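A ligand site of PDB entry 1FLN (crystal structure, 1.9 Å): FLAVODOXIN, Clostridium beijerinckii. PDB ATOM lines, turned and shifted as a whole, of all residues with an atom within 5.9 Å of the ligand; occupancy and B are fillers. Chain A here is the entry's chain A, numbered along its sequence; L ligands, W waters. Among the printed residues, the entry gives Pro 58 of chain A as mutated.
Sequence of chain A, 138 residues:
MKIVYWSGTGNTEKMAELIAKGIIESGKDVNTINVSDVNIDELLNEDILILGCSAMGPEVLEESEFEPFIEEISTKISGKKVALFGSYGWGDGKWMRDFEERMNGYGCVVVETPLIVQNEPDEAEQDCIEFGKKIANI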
ATOM      1  N   TRP A   6     -11.935  19.725 -10.790  1.00  0.00           N
ATOM      2  CA  TRP A   6     -13.109  19.971  -9.981  1.00  0.00           C
ATOM      3  C   TRP A   6     -14.142  19.031 -10.613  1.00  0.00           C
ATOM      4  O   TRP A   6     -14.178  18.908 -11.833  1.00  0.00           O
ATOM      5  CB  TRP A   6     -13.605  21.420 -10.072  1.00  0.00           C
ATOM      6  CG  TRP A   6     -14.792  21.615  -9.141  1.00  0.00           C
ATOM      7  CD1 TRP A   6     -14.748  21.859  -7.799  1.00  0.00           C
ATOM      8  CD2 TRP A   6     -16.179  21.424  -9.480  1.00  0.00           C
ATOM      9  NE1 TRP A   6     -16.024  21.820  -7.277  1.00  0.00           N
ATOM     10  CE2 TRP A   6     -16.919  21.554  -8.273  1.00  0.00           C
ATOM     11  CE3 TRP A   6     -16.870  21.149 -10.665  1.00  0.00           C
ATOM     12  CZ2 TRP A   6     -18.321  21.413  -8.240  1.00  0.00           C
ATOM     13  CZ3 TRP A   6     -18.263  21.008 -10.627  1.00  0.00           C
ATOM     14  CH2 TRP A   6     -18.962  21.148  -9.413  1.00  0.00           C
ATOM     15  N   SER A   7     -14.948  18.359  -9.800  1.00  0.00           N
ATOM     16  CA  SER A   7     -15.985  17.458 -10.308  1.00  0.00           C
ATOM     17  C   SER A   7     -17.171  17.516  -9.339  1.00  0.00           C
ATOM     18  O   SER A   7     -16.995  17.441  -8.108  1.00  0.00           O
ATOM     19  CB  SER A   7     -15.435  16.042 -10.428  1.00  0.00           C
ATOM     20  OG  SER A   7     -16.357  15.142 -11.023  1.00  0.00           O
ATOM     21  N   GLY A   8     -18.370  17.699  -9.892  1.00  0.00           N
ATOM     22  CA  GLY A   8     -19.568  17.795  -9.085  1.00  0.00           C
ATOM     23  C   GLY A   8     -20.291  16.486  -8.857  1.00  0.00           C
ATOM     24  O   GLY A   8     -20.922  16.297  -7.806  1.00  0.00           O
ATOM     25  N   THR A   9     -20.238  15.578  -9.825  1.00  0.00           N
ATOM     26  CA  THR A   9     -20.898  14.284  -9.672  1.00  0.00           C
ATOM     27  C   THR A   9     -19.916  13.106  -9.818  1.00  0.00           C
ATOM     28  O   THR A   9     -20.283  11.963  -9.598  1.00  0.00           O
ATOM     29  CB  THR A   9     -22.106  14.098 -10.626  1.00  0.00           C
ATOM     30  OG1 THR A   9     -21.651  13.877 -11.961  1.00  0.00           O
ATOM     31  CG2 THR A   9     -23.005  15.329 -10.611  1.00  0.00           C
ATOM     32  N   GLY A  10     -18.681  13.411 -10.197  1.00  0.00           N
ATOM     33  CA  GLY A  10     -17.689  12.365 -10.356  1.00  0.00           C
ATOM     34  C   GLY A  10     -17.270  12.071 -11.787  1.00  0.00           C
ATOM     35  O   GLY A  10     -16.355  11.288 -11.996  1.00  0.00           O
ATOM     36  N   ASN A  11     -17.883  12.730 -12.768  1.00  0.00           N
ATOM     37  CA  ASN A  11     -17.550  12.475 -14.164  1.00  0.00           C
ATOM     38  C   ASN A  11     -16.135  12.924 -14.546  1.00  0.00           C
ATOM     39  O   ASN A  11     -15.363  12.148 -15.134  1.00  0.00           O
ATOM     40  CB  ASN A  11     -18.587  13.086 -15.114  1.00  0.00           C
ATOM     41  CG  ASN A  11     -19.916  12.379 -15.032  1.00  0.00           C
ATOM     42  OD1 ASN A  11     -20.950  12.923 -15.413  1.00  0.00           O
ATOM     43  ND2 ASN A  11     -19.902  11.160 -14.531  1.00  0.00           N
ATOM     44  N   THR A  12     -15.801  14.163 -14.211  1.00  0.00           N
ATOM     45  CA  THR A  12     -14.466  14.714 -14.488  1.00  0.00           C
ATOM     46  C   THR A  12     -13.439  14.023 -13.594  1.00  0.00           C
ATOM     47  O   THR A  12     -12.310  13.820 -14.009  1.00  0.00           O
ATOM     48  CB  THR A  12     -14.429  16.255 -14.265  1.00  0.00           C
ATOM     49  OG1 THR A  12     -15.367  16.865 -15.166  1.00  0.00           O
ATOM     50  CG2 THR A  12     -13.043  16.819 -14.563  1.00  0.00           C
ATOM     51  N   GLU A  13     -13.865  13.625 -12.395  1.00  0.00           N
ATOM     52  CA  GLU A  13     -12.971  12.927 -11.472  1.00  0.00           C
ATOM     53  C   GLU A  13     -12.540  11.584 -12.070  1.00  0.00           C
ATOM     54  O   GLU A  13     -11.371  11.189 -11.965  1.00  0.00           O
ATOM     55  CB  GLU A  13     -13.642  12.682 -10.110  1.00  0.00           C
ATOM     56  CG  GLU A  13     -12.703  12.030  -9.099  1.00  0.00           C
ATOM     57  CD  GLU A  13     -13.362  11.621  -7.792  1.00  0.00           C
ATOM     58  OE1 GLU A  13     -14.606  11.672  -7.674  1.00  0.00           O
ATOM     59  OE2 GLU A  13     -12.632  11.198  -6.873  1.00  0.00           O
ATOM     60  N   SER A  54     -15.676  20.322 -15.262  1.00  0.00           N
ATOM     61  CA  SER A  54     -16.876  20.094 -16.046  1.00  0.00           C
ATOM     62  C   SER A  54     -17.516  21.423 -16.452  1.00  0.00           C
ATOM     63  O   SER A  54     -17.203  22.490 -15.893  1.00  0.00           O
ATOM     64  CB  SER A  54     -17.868  19.299 -15.199  1.00  0.00           C
ATOM     65  OG  SER A  54     -18.020  19.896 -13.940  1.00  0.00           O
ATOM     66  N   ALA A  55     -18.422  21.347 -17.428  1.00  0.00           N
ATOM     67  CA  ALA A  55     -19.116  22.541 -17.898  1.00  0.00           C
ATOM     68  C   ALA A  55     -20.156  22.849 -16.832  1.00  0.00           C
ATOM     69  O   ALA A  55     -20.986  22.000 -16.493  1.00  0.00           O
ATOM     70  CB  ALA A  55     -19.785  22.263 -19.230  1.00  0.00           C
ATOM     71  N   MET A  56     -20.086  24.050 -16.260  1.00  0.00           N
ATOM     72  CA  MET A  56     -21.015  24.449 -15.200  1.00  0.00           C
ATOM     73  C   MET A  56     -21.752  25.751 -15.526  1.00  0.00           C
ATOM     74  O   MET A  56     -21.470  26.390 -16.538  1.00  0.00           O
ATOM     75  CB  MET A  56     -20.273  24.554 -13.881  1.00  0.00           C
ATOM     76  CG  MET A  56     -19.869  23.199 -13.305  1.00  0.00           C
ATOM     77  SD  MET A  56     -21.310  22.189 -12.850  1.00  0.00           S
ATOM     78  CE  MET A  56     -21.867  23.065 -11.472  1.00  0.00           C
ATOM     79  N   GLY A  57     -22.729  26.091 -14.691  1.00  0.00           N
ATOM     80  CA  GLY A  57     -23.530  27.291 -14.891  1.00  0.00           C
ATOM     81  C   GLY A  57     -23.907  27.512 -16.335  1.00  0.00           C
ATOM     82  O   GLY A  57     -24.316  26.577 -17.016  1.00  0.00           O
ATOM     83  N   PRO A  58     -23.863  28.755 -16.825  1.00  0.00           N
ATOM     84  CA  PRO A  58     -24.202  29.037 -18.224  1.00  0.00           C
ATOM     85  C   PRO A  58     -22.948  28.843 -19.107  1.00  0.00           C
ATOM     86  O   PRO A  58     -22.397  29.823 -19.624  1.00  0.00           O
ATOM     87  CB  PRO A  58     -24.630  30.506 -18.174  1.00  0.00           C
ATOM     88  CG  PRO A  58     -23.733  31.072 -17.120  1.00  0.00           C
ATOM     89  CD  PRO A  58     -23.739  29.998 -16.035  1.00  0.00           C
ATOM     90  N   GLU A  59     -22.521  27.594 -19.294  1.00  0.00           N
ATOM     91  CA  GLU A  59     -21.323  27.257 -20.081  1.00  0.00           C
ATOM     92  C   GLU A  59     -20.079  27.983 -19.596  1.00  0.00           C
ATOM     93  O   GLU A  59     -19.405  28.648 -20.379  1.00  0.00           O
ATOM     94  CB  GLU A  59     -21.471  27.565 -21.573  1.00  0.00           C
ATOM     95  CG  GLU A  59     -22.305  26.620 -22.382  1.00  0.00           C
ATOM     96  CD  GLU A  59     -21.736  25.238 -22.607  1.00  0.00           C
ATOM     97  OE1 GLU A  59     -20.517  24.983 -22.508  1.00  0.00           O
ATOM     98  OE2 GLU A  59     -22.544  24.384 -22.948  1.00  0.00           O
ATOM     99  N   VAL A  60     -19.757  27.823 -18.319  1.00  0.00           N
ATOM    100  CA  VAL A  60     -18.588  28.467 -17.738  1.00  0.00           C
ATOM    101  C   VAL A  60     -17.864  27.471 -16.839  1.00  0.00           C
ATOM    102  O   VAL A  60     -18.340  26.343 -16.627  1.00  0.00           O
ATOM    103  CB  VAL A  60     -18.982  29.712 -16.892  1.00  0.00           C
ATOM    104  CG1 VAL A  60     -19.591  30.792 -17.776  1.00  0.00           C
ATOM    105  CG2 VAL A  60     -19.974  29.315 -15.784  1.00  0.00           C
ATOM    106  N   SER A  87     -15.742  16.985 -18.453  1.00  0.00           N
ATOM    107  CA  SER A  87     -16.982  16.358 -18.875  1.00  0.00           C
ATOM    108  C   SER A  87     -18.035  17.448 -19.071  1.00  0.00           C
ATOM    109  O   SER A  87     -17.975  18.508 -18.432  1.00  0.00           O
ATOM    110  CB  SER A  87     -17.462  15.374 -17.814  1.00  0.00           C
ATOM    111  OG  SER A  87     -18.675  14.752 -18.200  1.00  0.00           O
ATOM    112  N   TYR A  88     -19.028  17.182 -19.915  1.00  0.00           N
ATOM    113  CA  TYR A  88     -20.073  18.152 -20.168  1.00  0.00           C
ATOM    114  C   TYR A  88     -21.396  17.426 -20.399  1.00  0.00           C
ATOM    115  O   TYR A  88     -21.417  16.195 -20.520  1.00  0.00           O
ATOM    116  CB  TYR A  88     -19.739  19.064 -21.354  1.00  0.00           C
ATOM    117  CG  TYR A  88     -19.662  18.351 -22.687  1.00  0.00           C
ATOM    118  CD1 TYR A  88     -18.548  17.579 -23.028  1.00  0.00           C
ATOM    119  CD2 TYR A  88     -20.689  18.477 -23.618  1.00  0.00           C
ATOM    120  CE1 TYR A  88     -18.455  16.947 -24.244  1.00  0.00           C
ATOM    121  CE2 TYR A  88     -20.608  17.838 -24.853  1.00  0.00           C
ATOM    122  CZ  TYR A  88     -19.500  17.086 -25.163  1.00  0.00           C
ATOM    123  OH  TYR A  88     -19.416  16.466 -26.387  1.00  0.00           O
ATOM    124  N   GLY A  89     -22.481  18.180 -20.446  1.00  0.00           N
ATOM    125  CA  GLY A  89     -23.784  17.563 -20.603  1.00  0.00           C
ATOM    126  C   GLY A  89     -24.489  17.797 -21.903  1.00  0.00           C
ATOM    127  O   GLY A  89     -24.346  17.012 -22.834  1.00  0.00           O
ATOM    128  N   TRP A  90     -25.196  18.914 -21.991  1.00  0.00           N
ATOM    129  CA  TRP A  90     -26.002  19.246 -23.162  1.00  0.00           C
ATOM    130  C   TRP A  90     -25.391  20.147 -24.226  1.00  0.00           C
ATOM    131  O   TRP A  90     -25.939  20.270 -25.324  1.00  0.00           O
ATOM    132  CB  TRP A  90     -27.330  19.855 -22.711  1.00  0.00           C
ATOM    133  CG  TRP A  90     -27.164  21.004 -21.764  1.00  0.00           C
ATOM    134  CD1 TRP A  90     -26.950  22.319 -22.084  1.00  0.00           C
ATOM    135  CD2 TRP A  90     -27.224  20.955 -20.324  1.00  0.00           C
ATOM    136  NE1 TRP A  90     -26.875  23.085 -20.939  1.00  0.00           N
ATOM    137  CE2 TRP A  90     -27.037  22.274 -19.851  1.00  0.00           C
ATOM    138  CE3 TRP A  90     -27.407  19.912 -19.396  1.00  0.00           C
ATOM    139  CZ2 TRP A  90     -27.045  22.582 -18.484  1.00  0.00           C
ATOM    140  CZ3 TRP A  90     -27.412  20.224 -18.038  1.00  0.00           C
ATOM    141  CH2 TRP A  90     -27.234  21.553 -17.597  1.00  0.00           C
ATOM    142  N   GLY A  91     -24.296  20.818 -23.884  1.00  0.00           N
ATOM    143  CA  GLY A  91     -23.672  21.720 -24.826  1.00  0.00           C
ATOM    144  C   GLY A  91     -22.788  20.988 -25.810  1.00  0.00           C
ATOM    145  O   GLY A  91     -22.831  19.752 -25.906  1.00  0.00           O
ATOM    146  N   ASP A  92     -21.978  21.747 -26.531  1.00  0.00           N
ATOM    147  CA  ASP A  92     -21.059  21.172 -27.493  1.00  0.00           C
ATOM    148  C   ASP A  92     -19.614  21.610 -27.256  1.00  0.00           C
ATOM    149  O   ASP A  92     -18.836  21.770 -28.208  1.00  0.00           O
ATOM    150  CB  ASP A  92     -21.506  21.453 -28.945  1.00  0.00           C
ATOM    151  CG  ASP A  92     -21.563  22.948 -29.275  1.00  0.00           C
ATOM    152  OD1 ASP A  92     -20.945  23.780 -28.568  1.00  0.00           O
ATOM    153  OD2 ASP A  92     -22.219  23.273 -30.286  1.00  0.00           O
ATOM    154  N   GLY A  93     -19.271  21.878 -26.003  1.00  0.00           N
ATOM    155  CA  GLY A  93     -17.908  22.249 -25.688  1.00  0.00           C
ATOM    156  C   GLY A  93     -17.600  23.715 -25.638  1.00  0.00           C
ATOM    157  O   GLY A  93     -16.434  24.071 -25.545  1.00  0.00           O
ATOM    158  N   TRP A  95     -17.756  25.947 -23.180  1.00  0.00           N
ATOM    159  CA  TRP A  95     -16.960  26.317 -22.014  1.00  0.00           C
ATOM    160  C   TRP A  95     -15.474  25.949 -22.191  1.00  0.00           C
ATOM    161  O   TRP A  95     -14.604  26.661 -21.698  1.00  0.00           O
ATOM    162  CB  TRP A  95     -17.539  25.694 -20.726  1.00  0.00           C
ATOM    163  CG  TRP A  95     -16.821  24.440 -20.195  1.00  0.00           C
ATOM    164  CD1 TRP A  95     -16.078  24.331 -19.043  1.00  0.00           C
ATOM    165  CD2 TRP A  95     -16.792  23.142 -20.814  1.00  0.00           C
ATOM    166  NE1 TRP A  95     -15.600  23.049 -18.909  1.00  0.00           N
ATOM    167  CE2 TRP A  95     -16.018  22.295 -19.974  1.00  0.00           C
ATOM    168  CE3 TRP A  95     -17.342  22.593 -21.991  1.00  0.00           C
ATOM    169  CZ2 TRP A  95     -15.774  20.945 -20.269  1.00  0.00           C
ATOM    170  CZ3 TRP A  95     -17.109  21.250 -22.285  1.00  0.00           C
ATOM    171  CH2 TRP A  95     -16.327  20.442 -21.423  1.00  0.00           C
ATOM    172  N   VAL A 117     -15.536  14.953 -22.773  1.00  0.00           N
ATOM    173  CA  VAL A 117     -16.351  13.745 -22.870  1.00  0.00           C
ATOM    174  C   VAL A 117     -17.740  14.060 -22.342  1.00  0.00           C
ATOM    175  O   VAL A 117     -17.871  14.751 -21.335  1.00  0.00           O
ATOM    176  CB  VAL A 117     -15.747  12.604 -22.006  1.00  0.00           C
ATOM    177  CG1 VAL A 117     -16.699  11.430 -21.924  1.00  0.00           C
ATOM    178  CG2 VAL A 117     -14.414  12.162 -22.594  1.00  0.00           C
ATOM    179  N   GLN A 118     -18.769  13.559 -23.011  1.00  0.00           N
ATOM    180  CA  GLN A 118     -20.128  13.814 -22.562  1.00  0.00           C
ATOM    181  C   GLN A 118     -20.512  12.861 -21.450  1.00  0.00           C
ATOM    182  O   GLN A 118     -20.407  11.641 -21.613  1.00  0.00           O
ATOM    183  CB  GLN A 118     -21.121  13.672 -23.721  1.00  0.00           C
ATOM    184  CG  GLN A 118     -22.540  14.087 -23.355  1.00  0.00           C
ATOM    185  CD  GLN A 118     -23.527  13.955 -24.506  1.00  0.00           C
ATOM    186  OE1 GLN A 118     -23.322  14.524 -25.571  1.00  0.00           O
ATOM    187  NE2 GLN A 118     -24.604  13.201 -24.283  1.00  0.00           N
ATOM    188  N   ASN A 119     -20.952  13.413 -20.321  1.00  0.00           N
ATOM    189  CA  ASN A 119     -21.352  12.618 -19.171  1.00  0.00           C
ATOM    190  C   ASN A 119     -20.191  11.747 -18.684  1.00  0.00           C
ATOM    191  O   ASN A 119     -19.027  12.139 -18.798  1.00  0.00           O
ATOM    192  CB  ASN A 119     -22.597  11.783 -19.523  1.00  0.00           C
ATOM    193  CG  ASN A 119     -23.703  12.627 -20.180  1.00  0.00           C
ATOM    194  OD1 ASN A 119     -24.171  13.618 -19.596  1.00  0.00           O
ATOM    195  ND2 ASN A 119     -24.067  12.277 -21.412  1.00  0.00           N
ATOM    196  N   GLU A 120     -20.483  10.568 -18.147  1.00  0.00           N
ATOM    197  CA  GLU A 120     -19.431   9.673 -17.653  1.00  0.00           C
ATOM    198  C   GLU A 120     -18.604   9.065 -18.797  1.00  0.00           C
ATOM    199  O   GLU A 120     -19.168   8.682 -19.812  1.00  0.00           O
ATOM    200  CB  GLU A 120     -20.067   8.542 -16.819  1.00  0.00           C
ATOM    201  CG  GLU A 120     -19.067   7.701 -16.046  1.00  0.00           C
ATOM    202  CD  GLU A 120     -19.693   6.529 -15.300  1.00  0.00           C
ATOM    203  OE1 GLU A 120     -20.944   6.464 -15.231  1.00  0.00           O
ATOM    204  OE2 GLU A 120     -18.923   5.684 -14.779  1.00  0.00           O
HETATM  205  N1  LIG L   1     -23.280  20.874 -19.397  1.00  0.00           N
HETATM  206  C1  LIG L   1     -23.067  21.516 -20.528  1.00  0.00           C
HETATM  207  O1  LIG L   1     -22.861  20.900 -21.529  1.00  0.00           O
HETATM  208  N2  LIG L   1     -23.096  22.931 -20.547  1.00  0.00           N
HETATM  209  C2  LIG L   1     -23.497  23.730 -19.479  1.00  0.00           C
HETATM  210  O2  LIG L   1     -23.651  24.954 -19.533  1.00  0.00           O
HETATM  211  C3  LIG L   1     -23.756  22.987 -18.239  1.00  0.00           C
HETATM  212  N3  LIG L   1     -24.159  23.655 -17.179  1.00  0.00           N
HETATM  213  C4  LIG L   1     -24.450  22.933 -16.047  1.00  0.00           C
HETATM  214  C5  LIG L   1     -24.966  23.626 -14.910  1.00  0.00           C
HETATM  215  C6  LIG L   1     -25.240  22.972 -13.737  1.00  0.00           C
HETATM  216  C7  LIG L   1     -25.781  23.719 -12.559  1.00  0.00           C
HETATM  217  C8  LIG L   1     -25.008  21.572 -13.660  1.00  0.00           C
HETATM  218  C9  LIG L   1     -25.235  20.790 -12.380  1.00  0.00           C
HETATM  219  C10 LIG L   1     -24.545  20.889 -14.776  1.00  0.00           C
HETATM  220  C11 LIG L   1     -24.232  21.550 -15.966  1.00  0.00           C
HETATM  221  N4  LIG L   1     -23.829  20.889 -17.128  1.00  0.00           N
HETATM  222  C12 LIG L   1     -23.598  21.544 -18.306  1.00  0.00           C
HETATM  223  C13 LIG L   1     -23.741  19.436 -17.108  1.00  0.00           C
HETATM  224  C14 LIG L   1     -22.371  18.918 -16.625  1.00  0.00           C
HETATM  225  O3  LIG L   1     -21.306  19.550 -17.339  1.00  0.00           O
HETATM  226  C15 LIG L   1     -22.298  17.417 -16.834  1.00  0.00           C
HETATM  227  O4  LIG L   1     -23.360  16.777 -16.124  1.00  0.00           O
HETATM  228  C16 LIG L   1     -20.957  16.758 -16.468  1.00  0.00           C
HETATM  229  O5  LIG L   1     -21.025  15.359 -16.761  1.00  0.00           O
HETATM  230  C17 LIG L   1     -20.688  16.877 -14.976  1.00  0.00           C
HETATM  231  O6  LIG L   1     -19.377  16.389 -14.641  1.00  0.00           O
HETATM  232  P1  LIG L   1     -18.862  16.390 -13.175  1.00  0.00           P
HETATM  233  O7  LIG L   1     -17.426  16.153 -13.328  1.00  0.00           O
HETATM  234  O8  LIG L   1     -19.278  17.643 -12.510  1.00  0.00           O
HETATM  235  O9  LIG L   1     -19.458  15.213 -12.420  1.00  0.00           O
HETATM  236  O   HOH W   1     -23.876  14.255 -17.078  1.00  0.00           O
HETATM  237  O   HOH W   2     -21.612  18.569 -11.754  1.00  0.00           O
HETATM  238  O   HOH W   3     -23.607  17.646 -13.360  1.00  0.00           O
HETATM  239  O   HOH W   4     -20.484  22.127 -23.415  1.00  0.00           O
HETATM  240  O   HOH W   5     -25.945  25.974 -20.236  1.00  0.00           O
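The backbone NH (N) of Ala 55 lies within hydrogen-bond range of the backbone carbonyl oxygen (O) of Ser 87. The side-chain hydroxyl (OG) of Ser 7 lies within hydrogen-bond range of the backbone NH (N) of Asn 11, 3.3 Å away. N of Gly 10 sits at hydrogen-bond distance from OG of Ser 7 (3.0 Å). N of Glu 13 is in hydrogen-bond range of OG of Ser 7. The backbone carbonyl oxygen (O) of Asn 119 is in hydrogen-bond range of the side-chain hydroxyl (OG) of Ser 87, at 2.7 Å. OG of Ser 87 sits close to O of Val 117 (3.2 Å). The indole nitrogen (NE1) of Trp 95 is in hydrogen-bond range of the backbone carbonyl oxygen (O) of Ser 54, at 3.5 Å. The side-chain amide nitrogen of Asn 119 lies close to the side-chain amide nitrogen of Gln 118, 3.1 Å away.
Water W5 bridges an oxygen (O2) of the ligand and the indole nitrogen (NE1) of Trp 90. Water W2 bridges O8 of the ligand and SD of Met 56. Water W1 bridges OD1 of Asn 119 (2.6 Å) and O4 of the ligand (2.7 Å). Water W4 lies within hydrogen-bond range of N of Gly 93 (2.9 Å), OE1 of Glu 59 (3.0 Å), O1 of the ligand (3.3 Å) and N of Asp 92 (3.5 Å).
The backbone carbonyl oxygen (O) of Gly 57 lies close to a nitrogen (N3) of the ligand (2.9 Å). Residues that only touch the ligand: Tyr 88, Met 56, Asn 119, Pro 58 and Trp 6. Hydrophobic or aromatic side chains that line the ligand: Trp 6, Ala 55, Met 56, Tyr 88 and Trp 90. Within 4 Å of the ligand: Trp 6, Ser 7, Gly 8, Thr 9, Gly 10, Asn 11, Thr 12, Ser 54, Ala 55, Met 56, Gly 57, Pro 58, Glu 59, Ser 87, Tyr 88, Gly 89, Trp 90, Gly 91 and Asn 119. The nearest printed residue that does not touch the ligand is Glu 13 (4.5 Å).
N of Thr 9 is in hydrogen-bond range of O9 of the ligand (2.7 Å). The side-chain hydroxyl of Thr 9 is in hydrogen-bond range of an oxygen (O9) of the ligand. N of Ala 55 is in hydrogen-bond range of O3 of the ligand (3.4 Å). The backbone carbonyl oxygen (O) of Ala 55 sits at hydrogen-bond distance from an oxygen (O3) of the ligand, at 2.6 Å. The backbone NH (N) of Thr 12 is in hydrogen-bond range of an oxygen (O7) of the ligand, 2.7 Å away. O7 of the ligand is in hydrogen-bond range of OG1 of Thr 12, at 2.9 Å. The side-chain hydroxyl of Ser 7 lies within hydrogen-bond range of an oxygen (O7) of the ligand (2.7 Å). An oxygen (O1) of the ligand is in hydrogen-bond range of the backbone NH (N) of Gly 91. The backbone NH (N) of Gly 8 sits at hydrogen-bond distance from an oxygen (O8) of the ligand (2.8 Å). The backbone NH of Asn 11 sits at hydrogen-bond distance from an oxygen (O9) of the ligand, 3.0 Å away. The side-chain amide oxygen (OD1) of Asn 11 lies within hydrogen-bond range of an oxygen (O5) of the ligand (2.8 Å). O5 of the ligand sits at hydrogen-bond distance from OG of Ser 87 (2.8 Å). The backbone NH of Glu 59 lies within hydrogen-bond range of an oxygen (O2) of the ligand (2.9 Å). OE2 of Glu 59 is in hydrogen-bond range of N2 of the ligand (2.9 Å). An oxygen (O8) of the ligand sits at hydrogen-bond distance from the side-chain hydroxyl (OG) of Ser 54 (3.0 Å). The backbone NH of Gly 89 sits at hydrogen-bond distance from an oxygen (O1) of the ligand (3.0 Å). The backbone NH (N) of Gly 10 lies within hydrogen-bond range of an oxygen (O9) of the ligand (3.0 Å). N of Trp 90 lies within hydrogen-bond range of O1 of the ligand (3.1 Å).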
